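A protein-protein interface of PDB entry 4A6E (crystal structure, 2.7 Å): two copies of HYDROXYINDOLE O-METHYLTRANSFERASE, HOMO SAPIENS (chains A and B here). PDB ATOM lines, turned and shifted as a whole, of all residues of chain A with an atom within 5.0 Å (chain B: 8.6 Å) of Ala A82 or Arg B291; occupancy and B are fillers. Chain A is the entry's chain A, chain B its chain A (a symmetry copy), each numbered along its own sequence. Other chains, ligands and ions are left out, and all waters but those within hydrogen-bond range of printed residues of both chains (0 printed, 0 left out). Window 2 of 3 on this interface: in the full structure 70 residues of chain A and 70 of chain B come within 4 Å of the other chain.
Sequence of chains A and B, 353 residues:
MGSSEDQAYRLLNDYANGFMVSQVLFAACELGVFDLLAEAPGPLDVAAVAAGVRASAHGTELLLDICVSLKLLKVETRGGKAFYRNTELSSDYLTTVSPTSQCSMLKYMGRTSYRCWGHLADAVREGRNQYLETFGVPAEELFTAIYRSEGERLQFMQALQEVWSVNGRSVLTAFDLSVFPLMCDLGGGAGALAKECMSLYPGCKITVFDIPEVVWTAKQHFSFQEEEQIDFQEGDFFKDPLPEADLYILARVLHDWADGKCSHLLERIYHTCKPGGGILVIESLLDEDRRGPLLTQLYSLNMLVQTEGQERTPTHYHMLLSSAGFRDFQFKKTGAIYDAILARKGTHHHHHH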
ATOM      1  N   LEU A  44      31.767  26.452 -11.155  1.00  0.00           N
ATOM      2  CA  LEU A  44      32.534  25.442 -11.898  1.00  0.00           C
ATOM      3  C   LEU A  44      31.789  24.147 -12.179  1.00  0.00           C
ATOM      4  O   LEU A  44      31.071  23.664 -11.295  1.00  0.00           O
ATOM      5  CB  LEU A  44      33.806  25.071 -11.115  1.00  0.00           C
ATOM      6  CG  LEU A  44      34.856  26.131 -10.837  1.00  0.00           C
ATOM      7  CD1 LEU A  44      35.945  25.550  -9.989  1.00  0.00           C
ATOM      8  CD2 LEU A  44      35.464  26.669 -12.113  1.00  0.00           C
ATOM      9  N   ASP A  45      32.039  23.524 -13.367  1.00  0.00           N
ATOM     10  CA  ASP A  45      31.470  22.209 -13.659  1.00  0.00           C
ATOM     11  C   ASP A  45      32.353  21.107 -13.041  1.00  0.00           C
ATOM     12  O   ASP A  45      33.434  21.407 -12.526  1.00  0.00           O
ATOM     13  CB  ASP A  45      31.184  21.970 -15.160  1.00  0.00           C
ATOM     14  CG  ASP A  45      32.349  22.027 -16.142  1.00  0.00           C
ATOM     15  OD1 ASP A  45      33.505  21.855 -15.711  1.00  0.00           O
ATOM     16  OD2 ASP A  45      32.095  22.189 -17.355  1.00  0.00           O
ATOM     17  N   VAL A  46      31.882  19.838 -13.077  1.00  0.00           N
ATOM     18  CA  VAL A  46      32.599  18.676 -12.534  1.00  0.00           C
ATOM     19  C   VAL A  46      34.012  18.524 -13.129  1.00  0.00           C
ATOM     20  O   VAL A  46      34.962  18.345 -12.366  1.00  0.00           O
ATOM     21  CB  VAL A  46      31.763  17.367 -12.580  1.00  0.00           C
ATOM     22  CG1 VAL A  46      31.188  17.128 -13.964  1.00  0.00           C
ATOM     23  CG2 VAL A  46      32.573  16.160 -12.131  1.00  0.00           C
ATOM     24  N   ASP A  65      28.212  16.176  -5.474  1.00  0.00           N
ATOM     25  CA  ASP A  65      26.804  15.844  -5.309  1.00  0.00           C
ATOM     26  C   ASP A  65      26.403  15.570  -3.882  1.00  0.00           C
ATOM     27  O   ASP A  65      25.295  15.940  -3.500  1.00  0.00           O
ATOM     28  CB  ASP A  65      26.413  14.695  -6.215  1.00  0.00           C
ATOM     29  CG  ASP A  65      26.360  15.046  -7.692  1.00  0.00           C
ATOM     30  OD1 ASP A  65      26.382  16.255  -8.020  1.00  0.00           O
ATOM     31  OD2 ASP A  65      26.280  14.110  -8.520  1.00  0.00           O
ATOM     32  N   VAL A  68      26.279  18.998  -1.980  1.00  0.00           N
ATOM     33  CA  VAL A  68      25.032  19.686  -2.354  1.00  0.00           C
ATOM     34  C   VAL A  68      23.888  19.166  -1.461  1.00  0.00           C
ATOM     35  O   VAL A  68      23.140  19.962  -0.892  1.00  0.00           O
ATOM     36  CB  VAL A  68      24.718  19.517  -3.859  1.00  0.00           C
ATOM     37  CG1 VAL A  68      23.317  19.997  -4.189  1.00  0.00           C
ATOM     38  CG2 VAL A  68      25.737  20.250  -4.710  1.00  0.00           C
ATOM     39  N   SER A  69      23.790  17.835  -1.313  1.00  0.00           N
ATOM     40  CA  SER A  69      22.787  17.195  -0.471  1.00  0.00           C
ATOM     41  C   SER A  69      22.988  17.531   1.016  1.00  0.00           C
ATOM     42  O   SER A  69      22.012  17.648   1.758  1.00  0.00           O
ATOM     43  CB  SER A  69      22.771  15.689  -0.709  1.00  0.00           C
ATOM     44  OG  SER A  69      22.185  15.403  -1.969  1.00  0.00           O
ATOM     45  N   VAL A  75      24.068  24.003  -6.306  1.00  0.00           N
ATOM     46  CA  VAL A  75      24.215  23.647  -7.705  1.00  0.00           C
ATOM     47  C   VAL A  75      23.176  24.401  -8.542  1.00  0.00           C
ATOM     48  O   VAL A  75      22.044  24.607  -8.094  1.00  0.00           O
ATOM     49  CB  VAL A  75      24.149  22.101  -7.911  1.00  0.00           C
ATOM     50  CG1 VAL A  75      22.810  21.522  -7.461  1.00  0.00           C
ATOM     51  CG2 VAL A  75      24.459  21.691  -9.355  1.00  0.00           C
ATOM     52  N   GLU A  76      23.567  24.819  -9.748  1.00  0.00           N
ATOM     53  CA  GLU A  76      22.658  25.424 -10.722  1.00  0.00           C
ATOM     54  C   GLU A  76      22.870  24.742 -12.069  1.00  0.00           C
ATOM     55  O   GLU A  76      23.981  24.289 -12.362  1.00  0.00           O
ATOM     56  CB  GLU A  76      22.769  26.968 -10.800  1.00  0.00           C
ATOM     57  CG  GLU A  76      23.972  27.524 -11.551  1.00  0.00           C
ATOM     58  CD  GLU A  76      24.855  28.471 -10.759  1.00  0.00           C
ATOM     59  OE1 GLU A  76      25.466  28.032  -9.754  1.00  0.00           O
ATOM     60  OE2 GLU A  76      24.963  29.648 -11.175  1.00  0.00           O
ATOM     61  N   THR A  77      21.805  24.620 -12.856  1.00  0.00           N
ATOM     62  CA  THR A  77      21.889  24.016 -14.181  1.00  0.00           C
ATOM     63  C   THR A  77      22.025  25.115 -15.235  1.00  0.00           C
ATOM     64  O   THR A  77      21.303  26.117 -15.182  1.00  0.00           O
ATOM     65  CB  THR A  77      20.672  23.121 -14.462  1.00  0.00           C
ATOM     66  OG1 THR A  77      19.487  23.882 -14.210  1.00  0.00           O
ATOM     67  CG2 THR A  77      20.682  21.824 -13.644  1.00  0.00           C
ATOM     68  N   GLY A  80      23.225  21.727 -20.606  1.00  0.00           N
ATOM     69  CA  GLY A  80      23.139  20.359 -20.103  1.00  0.00           C
ATOM     70  C   GLY A  80      24.276  20.106 -19.121  1.00  0.00           C
ATOM     71  O   GLY A  80      25.005  19.112 -19.261  1.00  0.00           O
ATOM     72  N   LYS A  81      24.472  21.037 -18.147  1.00  0.00           N
ATOM     73  CA  LYS A  81      25.593  20.957 -17.212  1.00  0.00           C
ATOM     74  C   LYS A  81      25.358  21.543 -15.815  1.00  0.00           C
ATOM     75  O   LYS A  81      24.892  22.681 -15.660  1.00  0.00           O
ATOM     76  CB  LYS A  81      26.841  21.619 -17.834  1.00  0.00           C
ATOM     77  CG  LYS A  81      27.918  20.659 -18.324  1.00  0.00           C
ATOM     78  CD  LYS A  81      29.113  21.420 -18.922  1.00  0.00           C
ATOM     79  CE  LYS A  81      29.957  20.559 -19.841  1.00  0.00           C
ATOM     80  NZ  LYS A  81      29.262  20.223 -21.125  1.00  0.00           N
ATOM     81  N   ALA A  82      25.766  20.776 -14.803  1.00  0.00           N
ATOM     82  CA  ALA A  82      25.722  21.206 -13.418  1.00  0.00           C
ATOM     83  C   ALA A  82      26.966  22.032 -13.152  1.00  0.00           C
ATOM     84  O   ALA A  82      28.085  21.641 -13.529  1.00  0.00           O
ATOM     85  CB  ALA A  82      25.697  20.009 -12.488  1.00  0.00           C
ATOM     86  N   PHE A  83      26.745  23.191 -12.514  1.00  0.00           N
ATOM     87  CA  PHE A  83      27.751  24.133 -12.069  1.00  0.00           C
ATOM     88  C   PHE A  83      27.586  24.310 -10.578  1.00  0.00           C
ATOM     89  O   PHE A  83      26.467  24.476 -10.087  1.00  0.00           O
ATOM     90  CB  PHE A  83      27.629  25.449 -12.828  1.00  0.00           C
ATOM     91  CG  PHE A  83      28.114  25.300 -14.245  1.00  0.00           C
ATOM     92  CD1 PHE A  83      29.457  25.472 -14.557  1.00  0.00           C
ATOM     93  CD2 PHE A  83      27.240  24.938 -15.262  1.00  0.00           C
ATOM     94  CE1 PHE A  83      29.910  25.323 -15.870  1.00  0.00           C
ATOM     95  CE2 PHE A  83      27.694  24.783 -16.573  1.00  0.00           C
ATOM     96  CZ  PHE A  83      29.028  24.971 -16.868  1.00  0.00           C
ATOM     97  N   TYR A  84      28.698  24.210  -9.858  1.00  0.00           N
ATOM     98  CA  TYR A  84      28.739  24.265  -8.397  1.00  0.00           C
ATOM     99  C   TYR A  84      29.305  25.558  -7.909  1.00  0.00           C
ATOM    100  O   TYR A  84      30.172  26.144  -8.559  1.00  0.00           O
ATOM    101  CB  TYR A  84      29.532  23.072  -7.834  1.00  0.00           C
ATOM    102  CG  TYR A  84      28.981  21.737  -8.292  1.00  0.00           C
ATOM    103  CD1 TYR A  84      29.348  21.191  -9.524  1.00  0.00           C
ATOM    104  CD2 TYR A  84      28.037  21.052  -7.529  1.00  0.00           C
ATOM    105  CE1 TYR A  84      28.789  19.996  -9.984  1.00  0.00           C
ATOM    106  CE2 TYR A  84      27.475  19.853  -7.977  1.00  0.00           C
ATOM    107  CZ  TYR A  84      27.866  19.322  -9.198  1.00  0.00           C
ATOM    108  OH  TYR A  84      27.344  18.119  -9.611  1.00  0.00           O
ATOM    109  N   LEU B 286      19.188   5.289  -7.571  1.00  0.00           N
ATOM    110  CA  LEU B 286      19.621   6.670  -7.480  1.00  0.00           C
ATOM    111  C   LEU B 286      18.607   7.534  -8.216  1.00  0.00           C
ATOM    112  O   LEU B 286      18.094   7.110  -9.256  1.00  0.00           O
ATOM    113  CB  LEU B 286      20.990   6.755  -8.183  1.00  0.00           C
ATOM    114  CG  LEU B 286      22.097   7.687  -7.683  1.00  0.00           C
ATOM    115  CD1 LEU B 286      22.319   7.578  -6.182  1.00  0.00           C
ATOM    116  CD2 LEU B 286      23.385   7.367  -8.402  1.00  0.00           C
ATOM    117  N   ASP B 287      18.299   8.736  -7.683  1.00  0.00           N
ATOM    118  CA  ASP B 287      17.386   9.679  -8.346  1.00  0.00           C
ATOM    119  C   ASP B 287      18.017  10.050  -9.699  1.00  0.00           C
ATOM    120  O   ASP B 287      19.247  10.060  -9.821  1.00  0.00           O
ATOM    121  CB  ASP B 287      17.151  10.941  -7.494  1.00  0.00           C
ATOM    122  CG  ASP B 287      16.468  10.748  -6.139  1.00  0.00           C
ATOM    123  OD1 ASP B 287      15.834   9.689  -5.931  1.00  0.00           O
ATOM    124  OD2 ASP B 287      16.527  11.687  -5.303  1.00  0.00           O
ATOM    125  N   GLU B 288      17.187  10.305 -10.715  1.00  0.00           N
ATOM    126  CA  GLU B 288      17.644  10.602 -12.074  1.00  0.00           C
ATOM    127  C   GLU B 288      18.734  11.671 -12.258  1.00  0.00           C
ATOM    128  O   GLU B 288      19.497  11.606 -13.222  1.00  0.00           O
ATOM    129  CB  GLU B 288      16.468  10.787 -13.032  1.00  0.00           C
ATOM    130  CG  GLU B 288      15.789   9.481 -13.429  1.00  0.00           C
ATOM    131  CD  GLU B 288      16.561   8.457 -14.245  1.00  0.00           C
ATOM    132  OE1 GLU B 288      17.621   8.802 -14.815  1.00  0.00           O
ATOM    133  OE2 GLU B 288      16.090   7.299 -14.316  1.00  0.00           O
ATOM    134  N   ASP B 289      18.834  12.617 -11.318  1.00  0.00           N
ATOM    135  CA  ASP B 289      19.824  13.700 -11.336  1.00  0.00           C
ATOM    136  C   ASP B 289      21.092  13.342 -10.520  1.00  0.00           C
ATOM    137  O   ASP B 289      21.940  14.201 -10.265  1.00  0.00           O
ATOM    138  CB  ASP B 289      19.166  15.038 -10.912  1.00  0.00           C
ATOM    139  CG  ASP B 289      18.686  15.180  -9.467  1.00  0.00           C
ATOM    140  OD1 ASP B 289      18.872  14.230  -8.674  1.00  0.00           O
ATOM    141  OD2 ASP B 289      18.174  16.265  -9.117  1.00  0.00           O
ATOM    142  N   ARG B 290      21.205  12.046 -10.125  1.00  0.00           N
ATOM    143  CA  ARG B 290      22.299  11.454  -9.330  1.00  0.00           C
ATOM    144  C   ARG B 290      22.529  12.214  -7.990  1.00  0.00           C
ATOM    145  O   ARG B 290      23.536  11.990  -7.302  1.00  0.00           O
ATOM    146  CB  ARG B 290      23.607  11.390 -10.153  1.00  0.00           C
ATOM    147  CG  ARG B 290      23.554  10.608 -11.467  1.00  0.00           C
ATOM    148  CD  ARG B 290      24.800  10.901 -12.291  1.00  0.00           C
ATOM    149  NE  ARG B 290      24.794  10.224 -13.584  1.00  0.00           N
ATOM    150  CZ  ARG B 290      25.637  10.482 -14.582  1.00  0.00           C
ATOM    151  NH1 ARG B 290      26.562  11.427 -14.453  1.00  0.00           N
ATOM    152  NH2 ARG B 290      25.551   9.806 -15.722  1.00  0.00           N
ATOM    153  N   ARG B 291      21.594  13.111  -7.630  1.00  0.00           N
ATOM    154  CA  ARG B 291      21.732  13.959  -6.451  1.00  0.00           C
ATOM    155  C   ARG B 291      20.984  13.515  -5.192  1.00  0.00           C
ATOM    156  O   ARG B 291      20.876  14.278  -4.232  1.00  0.00           O
ATOM    157  CB  ARG B 291      21.475  15.428  -6.817  1.00  0.00           C
ATOM    158  CG  ARG B 291      22.548  16.388  -6.301  1.00  0.00           C
ATOM    159  CD  ARG B 291      22.607  17.656  -7.134  1.00  0.00           C
ATOM    160  NE  ARG B 291      23.342  17.430  -8.379  1.00  0.00           N
ATOM    161  CZ  ARG B 291      22.843  17.614  -9.595  1.00  0.00           C
ATOM    162  NH1 ARG B 291      21.599  18.051  -9.753  1.00  0.00           N
ATOM    163  NH2 ARG B 291      23.589  17.375 -10.662  1.00  0.00           N
ATOM    164  N   GLY B 292      20.556  12.261  -5.174  1.00  0.00           N
ATOM    165  CA  GLY B 292      19.868  11.674  -4.034  1.00  0.00           C
ATOM    166  C   GLY B 292      19.336  10.286  -4.318  1.00  0.00           C
ATOM    167  O   GLY B 292      19.376   9.831  -5.468  1.00  0.00           O
ATOM    168  N   PRO B 293      18.800   9.570  -3.306  1.00  0.00           N
ATOM    169  CA  PRO B 293      18.737   9.913  -1.871  1.00  0.00           C
ATOM    170  C   PRO B 293      20.154   9.907  -1.294  1.00  0.00           C
ATOM    171  O   PRO B 293      21.015   9.185  -1.821  1.00  0.00           O
ATOM    172  CB  PRO B 293      17.876   8.781  -1.269  1.00  0.00           C
ATOM    173  CG  PRO B 293      17.268   8.038  -2.448  1.00  0.00           C
ATOM    174  CD  PRO B 293      18.253   8.222  -3.561  1.00  0.00           C
ATOM    175  N   LEU B 294      20.414  10.738  -0.249  1.00  0.00           N
ATOM    176  CA  LEU B 294      21.727  10.878   0.377  1.00  0.00           C
ATOM    177  C   LEU B 294      22.310   9.533   0.763  1.00  0.00           C
ATOM    178  O   LEU B 294      23.510   9.316   0.527  1.00  0.00           O
ATOM    179  CB  LEU B 294      21.670  11.828   1.585  1.00  0.00           C
ATOM    180  CG  LEU B 294      22.883  11.933   2.519  1.00  0.00           C
ATOM    181  CD1 LEU B 294      24.130  12.463   1.800  1.00  0.00           C
ATOM    182  CD2 LEU B 294      22.565  12.821   3.701  1.00  0.00           C
ATOM    183  N   LEU B 295      21.477   8.616   1.333  1.00  0.00           N
ATOM    184  CA  LEU B 295      21.970   7.290   1.748  1.00  0.00           C
ATOM    185  C   LEU B 295      22.530   6.534   0.526  1.00  0.00           C
ATOM    186  O   LEU B 295      23.620   5.979   0.614  1.00  0.00           O
ATOM    187  CB  LEU B 295      20.880   6.482   2.495  1.00  0.00           C
ATOM    188  CG  LEU B 295      21.312   5.118   3.044  1.00  0.00           C
ATOM    189  CD1 LEU B 295      20.588   4.792   4.337  1.00  0.00           C
ATOM    190  CD2 LEU B 295      21.052   4.014   2.026  1.00  0.00           C
ATOM    191  N   THR B 296      21.791   6.550  -0.607  1.00  0.00           N
ATOM    192  CA  THR B 296      22.209   5.927  -1.864  1.00  0.00           C
ATOM    193  C   THR B 296      23.488   6.583  -2.389  1.00  0.00           C
ATOM    194  O   THR B 296      24.381   5.866  -2.852  1.00  0.00           O
ATOM    195  CB  THR B 296      21.077   5.923  -2.911  1.00  0.00           C
ATOM    196  OG1 THR B 296      19.850   5.520  -2.304  1.00  0.00           O
ATOM    197  CG2 THR B 296      21.378   5.017  -4.065  1.00  0.00           C
ATOM    198  N   GLN B 297      23.585   7.928  -2.310  1.00  0.00           N
ATOM    199  CA  GLN B 297      24.801   8.639  -2.730  1.00  0.00           C
ATOM    200  C   GLN B 297      26.047   8.151  -1.901  1.00  0.00           C
ATOM    201  O   GLN B 297      27.114   7.879  -2.467  1.00  0.00           O
ATOM    202  CB  GLN B 297      24.623  10.153  -2.573  1.00  0.00           C
ATOM    203  CG  GLN B 297      23.735  10.797  -3.604  1.00  0.00           C
ATOM    204  CD  GLN B 297      23.577  12.260  -3.314  1.00  0.00           C
ATOM    205  OE1 GLN B 297      22.892  12.664  -2.372  1.00  0.00           O
ATOM    206  NE2 GLN B 297      24.182  13.089  -4.132  1.00  0.00           N
ATOM    207  N   THR B 313      21.052   4.914 -11.691  1.00  0.00           N
ATOM    208  CA  THR B 313      19.699   5.470 -11.879  1.00  0.00           C
ATOM    209  C   THR B 313      18.855   4.465 -12.692  1.00  0.00           C
ATOM    210  O   THR B 313      19.448   3.709 -13.468  1.00  0.00           O
ATOM    211  CB  THR B 313      19.751   6.841 -12.622  1.00  0.00           C
ATOM    212  OG1 THR B 313      20.198   6.668 -13.971  1.00  0.00           O
ATOM    213  CG2 THR B 313      20.576   7.895 -11.893  1.00  0.00           C
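The side-chain carboxylate (OD1) of Asp A65 is in salt-bridge range of the guanidinium group (NE) of Arg B291. The backbone carbonyl oxygen (O) of Asp A65 is in hydrogen-bond range of the side-chain amide nitrogen (NE2) of Gln B297 (3.1 Å). O of Arg B291 lies within hydrogen-bond range of OG of Ser A69 (2.8 Å). OE1 of Gln B297 lies within hydrogen-bond range of OG of Ser A69, at 2.9 Å.
N of Tyr A84 sits at hydrogen-bond distance from O of Leu A44, at 2.8 Å. The side-chain hydroxyl (OH) of Tyr A84 is in hydrogen-bond range of the side-chain carboxylate (OD1) of Asp A65 (2.6 Å). The side-chain carboxylate of Asp B289 lies within salt-bridge range of the guanidinium group of Arg B291. NE2 of Gln B297 lies within hydrogen-bond range of O of Arg B290 (3.4 Å). OE1 of Gln B297 sits close to O of Arg B291.
Among the printed residues, merely in contact across the chains: Asp A65 with Arg B290 (3.7 Å), Val A68 with Arg B291 (3.8 Å), Val A75 with Arg B291 (3.9 Å), Ala A82 with Arg B291 (3.8 Å) and Tyr A84 with Arg B291 (3.97 Å).
Of the printed residues of chain B, Asp A65 touches Arg B290, Arg B291 and Gln B297. Of the printed residues of chain B, Ser A69 touches Arg B291 and Gln B297. Of chain B, only Arg B291 comes within 4 Å of Ala A82. Of the printed residues of chain B, Tyr A84 touches Arg B291. Of the printed residues of chain A, Gln B297 touches Asp A65 and Ser A69. The nearest residue of chain B that does not touch Ala A82 is Asp B289 (7.3 Å). The nearest printed residue of chain A that does not touch Arg B291 is Thr A77 (5.5 Å). The nearest printed residue of chain A that does not touch Arg B290 is Ser A69 (6.5 Å).
Of the 14 printed residues of chain A, 6 touch a printed residue of chain B. Among the printed residues, 9 pairs touch across the chains. Among the printed residues, Asp or Glu carboxylates within 4 Å of a Lys or Arg side-chain nitrogen of the other chain: Asp A65 with Arg B291.
No position is printed for both chains. Of the 9 pairs that touch across the chains among the printed residues, none has its exchanged pair printed and touching as well.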
